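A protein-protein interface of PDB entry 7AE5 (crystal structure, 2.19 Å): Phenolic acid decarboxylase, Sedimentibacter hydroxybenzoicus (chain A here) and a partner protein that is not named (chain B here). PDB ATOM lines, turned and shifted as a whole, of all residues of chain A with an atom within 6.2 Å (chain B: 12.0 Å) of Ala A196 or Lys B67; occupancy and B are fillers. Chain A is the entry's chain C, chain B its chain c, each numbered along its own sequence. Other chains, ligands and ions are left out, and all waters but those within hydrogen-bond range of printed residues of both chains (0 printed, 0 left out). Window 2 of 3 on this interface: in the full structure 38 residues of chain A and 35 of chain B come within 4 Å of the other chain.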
ATOM      1  N   LEU A 191       6.239  -0.680 -17.411  1.00  0.00           N
ATOM      2  CA  LEU A 191       5.551  -0.732 -18.695  1.00  0.00           C
ATOM      3  C   LEU A 191       5.118  -2.149 -19.048  1.00  0.00           C
ATOM      4  O   LEU A 191       4.020  -2.349 -19.579  1.00  0.00           O
ATOM      5  CB  LEU A 191       6.448  -0.162 -19.794  1.00  0.00           C
ATOM      6  CG  LEU A 191       5.824  -0.026 -21.181  1.00  0.00           C
ATOM      7  CD1 LEU A 191       4.476   0.671 -21.104  1.00  0.00           C
ATOM      8  CD2 LEU A 191       6.764   0.722 -22.102  1.00  0.00           C
ATOM      9  N   GLU A 192       5.970  -3.140 -18.774  1.00  0.00           N
ATOM     10  CA  GLU A 192       5.585  -4.527 -19.016  1.00  0.00           C
ATOM     11  C   GLU A 192       4.382  -4.915 -18.165  1.00  0.00           C
ATOM     12  O   GLU A 192       3.481  -5.619 -18.634  1.00  0.00           O
ATOM     13  CB  GLU A 192       6.767  -5.457 -18.739  1.00  0.00           C
ATOM     14  N   LYS A 193       4.345  -4.456 -16.912  1.00  0.00           N
ATOM     15  CA  LYS A 193       3.202  -4.743 -16.051  1.00  0.00           C
ATOM     16  C   LYS A 193       1.962  -3.986 -16.509  1.00  0.00           C
ATOM     17  O   LYS A 193       0.844  -4.509 -16.430  1.00  0.00           O
ATOM     18  CB  LYS A 193       3.537  -4.397 -14.601  1.00  0.00           C
ATOM     19  N   ALA A 194       2.138  -2.752 -16.990  1.00  0.00           N
ATOM     20  CA  ALA A 194       0.991  -1.957 -17.420  1.00  0.00           C
ATOM     21  C   ALA A 194       0.384  -2.508 -18.704  1.00  0.00           C
ATOM     22  O   ALA A 194      -0.844  -2.558 -18.845  1.00  0.00           O
ATOM     23  CB  ALA A 194       1.402  -0.497 -17.607  1.00  0.00           C
ATOM     24  N   GLU A 195       1.224  -2.926 -19.652  1.00  0.00           N
ATOM     25  CA  GLU A 195       0.710  -3.453 -20.910  1.00  0.00           C
ATOM     26  C   GLU A 195       0.190  -4.878 -20.760  1.00  0.00           C
ATOM     27  O   GLU A 195      -0.685  -5.296 -21.527  1.00  0.00           O
ATOM     28  CB  GLU A 195       1.793  -3.380 -21.989  1.00  0.00           C
ATOM     29  CG  GLU A 195       2.136  -1.951 -22.395  1.00  0.00           C
ATOM     30  CD  GLU A 195       3.026  -1.879 -23.621  1.00  0.00           C
ATOM     31  OE1 GLU A 195       4.128  -2.468 -23.598  1.00  0.00           O
ATOM     32  OE2 GLU A 195       2.623  -1.228 -24.609  1.00  0.00           O
ATOM     33  N   ALA A 196       0.703  -5.632 -19.785  1.00  0.00           N
ATOM     34  CA  ALA A 196       0.141  -6.949 -19.508  1.00  0.00           C
ATOM     35  C   ALA A 196      -1.250  -6.843 -18.898  1.00  0.00           C
ATOM     36  O   ALA A 196      -2.099  -7.709 -19.138  1.00  0.00           O
ATOM     37  CB  ALA A 196       1.067  -7.739 -18.584  1.00  0.00           C
ATOM     38  N   GLU A 197      -1.501  -5.795 -18.116  1.00  0.00           N
ATOM     39  CA  GLU A 197      -2.807  -5.547 -17.521  1.00  0.00           C
ATOM     40  C   GLU A 197      -3.638  -4.558 -18.328  1.00  0.00           C
ATOM     41  O   GLU A 197      -4.725  -4.175 -17.884  1.00  0.00           O
ATOM     42  CB  GLU A 197      -2.647  -5.046 -16.085  1.00  0.00           C
ATOM     43  CG  GLU A 197      -2.433  -6.151 -15.062  1.00  0.00           C
ATOM     44  CD  GLU A 197      -1.701  -5.669 -13.823  1.00  0.00           C
ATOM     45  OE1 GLU A 197      -1.634  -4.440 -13.610  1.00  0.00           O
ATOM     46  OE2 GLU A 197      -1.197  -6.521 -13.061  1.00  0.00           O
ATOM     47  N   ASN A 198      -3.145  -4.134 -19.495  1.00  0.00           N
ATOM     48  CA  ASN A 198      -3.873  -3.234 -20.393  1.00  0.00           C
ATOM     49  C   ASN A 198      -4.195  -1.904 -19.713  1.00  0.00           C
ATOM     50  O   ASN A 198      -5.269  -1.330 -19.905  1.00  0.00           O
ATOM     51  CB  ASN A 198      -5.146  -3.896 -20.925  1.00  0.00           C
ATOM     52  CG  ASN A 198      -5.507  -3.431 -22.321  1.00  0.00           C
ATOM     53  OD1 ASN A 198      -4.660  -2.934 -23.063  1.00  0.00           O
ATOM     54  ND2 ASN A 198      -6.773  -3.594 -22.688  1.00  0.00           N
ATOM     55  N   LYS A 199      -3.248  -1.404 -18.912  1.00  0.00           N
ATOM     56  CA  LYS A 199      -3.419  -0.160 -18.181  1.00  0.00           C
ATOM     57  C   LYS A 199      -2.527   0.936 -18.759  1.00  0.00           C
ATOM     58  O   LYS A 199      -1.452   0.654 -19.296  1.00  0.00           O
ATOM     59  CB  LYS A 199      -3.090  -0.341 -16.694  1.00  0.00           C
ATOM     60  CG  LYS A 199      -4.182  -1.031 -15.891  1.00  0.00           C
ATOM     61  CD  LYS A 199      -3.748  -1.264 -14.452  1.00  0.00           C
ATOM     62  CE  LYS A 199      -3.884   0.004 -13.623  1.00  0.00           C
ATOM     63  NZ  LYS A 199      -3.682  -0.252 -12.169  1.00  0.00           N
ATOM     64  N   ARG A 268      -0.084  -1.508 -25.210  1.00  0.00           N
ATOM     65  CA  ARG A 268      -0.145  -2.502 -26.283  1.00  0.00           C
ATOM     66  C   ARG A 268      -0.342  -1.876 -27.663  1.00  0.00           C
ATOM     67  O   ARG A 268      -0.944  -2.490 -28.546  1.00  0.00           O
ATOM     68  CB  ARG A 268      -1.242  -3.543 -26.022  1.00  0.00           C
ATOM     69  CG  ARG A 268      -1.361  -3.978 -24.570  1.00  0.00           C
ATOM     70  CD  ARG A 268      -2.398  -5.074 -24.399  1.00  0.00           C
ATOM     71  NE  ARG A 268      -2.146  -6.212 -25.273  1.00  0.00           N
ATOM     72  CZ  ARG A 268      -1.188  -7.107 -25.076  1.00  0.00           C
ATOM     73  NH1 ARG A 268      -0.361  -7.020 -24.047  1.00  0.00           N
ATOM     74  NH2 ARG A 268      -1.055  -8.116 -25.934  1.00  0.00           N
ATOM     75  N   PRO B  61       9.472  -1.618 -27.395  1.00  0.00           N
ATOM     76  CA  PRO B  61       9.880  -2.941 -26.915  1.00  0.00           C
ATOM     77  C   PRO B  61       8.812  -3.975 -27.277  1.00  0.00           C
ATOM     78  O   PRO B  61       7.763  -3.577 -27.784  1.00  0.00           O
ATOM     79  CB  PRO B  61       9.981  -2.740 -25.402  1.00  0.00           C
ATOM     80  CG  PRO B  61       8.947  -1.718 -25.119  1.00  0.00           C
ATOM     81  CD  PRO B  61       8.979  -0.774 -26.292  1.00  0.00           C
ATOM     82  N   PRO B  62       9.067  -5.263 -27.046  1.00  0.00           N
ATOM     83  CA  PRO B  62       8.040  -6.268 -27.351  1.00  0.00           C
ATOM     84  C   PRO B  62       6.816  -6.101 -26.462  1.00  0.00           C
ATOM     85  O   PRO B  62       6.920  -5.746 -25.285  1.00  0.00           O
ATOM     86  CB  PRO B  62       8.750  -7.602 -27.083  1.00  0.00           C
ATOM     87  CG  PRO B  62      10.206  -7.284 -27.127  1.00  0.00           C
ATOM     88  CD  PRO B  62      10.330  -5.887 -26.614  1.00  0.00           C
ATOM     89  N   ILE B  63       5.650  -6.353 -27.045  1.00  0.00           N
ATOM     90  CA  ILE B  63       4.390  -6.313 -26.307  1.00  0.00           C
ATOM     91  C   ILE B  63       4.236  -7.620 -25.540  1.00  0.00           C
ATOM     92  O   ILE B  63       4.145  -8.691 -26.157  1.00  0.00           O
ATOM     93  CB  ILE B  63       3.192  -6.084 -27.242  1.00  0.00           C
ATOM     94  CG1 ILE B  63       3.343  -4.768 -28.005  1.00  0.00           C
ATOM     95  CG2 ILE B  63       1.891  -6.094 -26.451  1.00  0.00           C
ATOM     96  CD1 ILE B  63       2.321  -4.591 -29.106  1.00  0.00           C
ATOM     97  N   PRO B  64       4.199  -7.587 -24.212  1.00  0.00           N
ATOM     98  CA  PRO B  64       4.001  -8.819 -23.445  1.00  0.00           C
ATOM     99  C   PRO B  64       2.598  -9.357 -23.654  1.00  0.00           C
ATOM    100  O   PRO B  64       1.699  -8.619 -24.084  1.00  0.00           O
ATOM    101  CB  PRO B  64       4.216  -8.366 -21.993  1.00  0.00           C
ATOM    102  CG  PRO B  64       3.846  -6.921 -22.003  1.00  0.00           C
ATOM    103  CD  PRO B  64       4.292  -6.400 -23.343  1.00  0.00           C
ATOM    104  N   PRO B  65       2.368 -10.638 -23.379  1.00  0.00           N
ATOM    105  CA  PRO B  65       1.008 -11.175 -23.476  1.00  0.00           C
ATOM    106  C   PRO B  65       0.133 -10.658 -22.344  1.00  0.00           C
ATOM    107  O   PRO B  65       0.609 -10.273 -21.274  1.00  0.00           O
ATOM    108  CB  PRO B  65       1.211 -12.690 -23.375  1.00  0.00           C
ATOM    109  CG  PRO B  65       2.488 -12.844 -22.623  1.00  0.00           C
ATOM    110  CD  PRO B  65       3.349 -11.675 -23.011  1.00  0.00           C
ATOM    111  N   LEU B  66      -1.172 -10.647 -22.604  1.00  0.00           N
ATOM    112  CA  LEU B  66      -2.126 -10.199 -21.602  1.00  0.00           C
ATOM    113  C   LEU B  66      -2.167 -11.176 -20.428  1.00  0.00           C
ATOM    114  O   LEU B  66      -1.830 -12.358 -20.553  1.00  0.00           O
ATOM    115  CB  LEU B  66      -3.518 -10.051 -22.215  1.00  0.00           C
ATOM    116  N   LYS B  67      -2.581 -10.664 -19.275  1.00  0.00           N
ATOM    117  CA  LYS B  67      -2.644 -11.471 -18.062  1.00  0.00           C
ATOM    118  C   LYS B  67      -4.081 -11.860 -17.732  1.00  0.00           C
ATOM    119  O   LYS B  67      -4.455 -13.030 -17.829  1.00  0.00           O
ATOM    120  CB  LYS B  67      -2.019 -10.717 -16.885  1.00  0.00           C
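N of Lys B67 is in hydrogen-bond range of O of Ala A196 (3.0 Å). NH1 of Arg A268 sits at hydrogen-bond distance from O of Pro B64 (2.6 Å).
The side-chain carboxylate of Glu A195 sits at hydrogen-bond distance from the backbone NH of Arg A268 (2.8 Å).
Glu A192 touches Pro B64 (O to CG, 3.6 Å). Pro B64 touches Glu A195. Ala A196 touches Pro B65. Ala A196 touches Leu B66 (O to CA, 3.5 Å). Ile B63 touches Arg A268 (CG2 to NH1, 3.4 Å). Arg A268 touches Leu B66 (NH1 to N, 3.99 Å).
Of chain B, only Pro B65 (3.7 Å), Leu B66 (3.5 Å) and Lys B67 (3.0 Å) come within 4 Å of Ala A196. Of the printed residues of chain B, Glu A192 touches Pro B64 (3.6 Å). No residue of chain B comes within 4 Å of Lys A193. Ala A194 touches none of the printed residues of chain B. Of chain B, only Pro B64 (3.9 Å) comes within 4 Å of Glu A195. No residue of chain B comes within 4 Å of Glu A197. Asn A198 touches none of the printed residues of chain B. Printed residues of chain A within 4 Å of Pro B64: Glu A192 (3.6 Å), Glu A195 (3.9 Å) and Arg A268 (2.6 Å). Of the printed residues of chain B, Arg A268 touches Ile B63 (3.4 Å), Pro B64 (2.6 Å) and Leu B66 (3.99 Å). The nearest printed residue of chain A that does not touch Pro B65 is Arg A268 (4.05 Å).
Printed residues of chain B that touch a printed residue of chain A: Ile B63, Pro B64, Pro B65, Leu B66 and Lys B67. Hydrophobic or aromatic side chains of chain B that line the printed part of chain A: Ile B63 and Pro B64. Along chain B the printed residues that touch a printed residue of chain A span positions 63 to 67. Of the 10 printed residues of chain A, 4 touch a printed residue of chain B. Hydrophobic or aromatic side chains of chain A within 4 Å of the printed part of chain B: Ala A196. Among the printed residues, no Asp or Glu carboxylate lies within 4 Å of a Lys or Arg side-chain nitrogen of the other chain.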
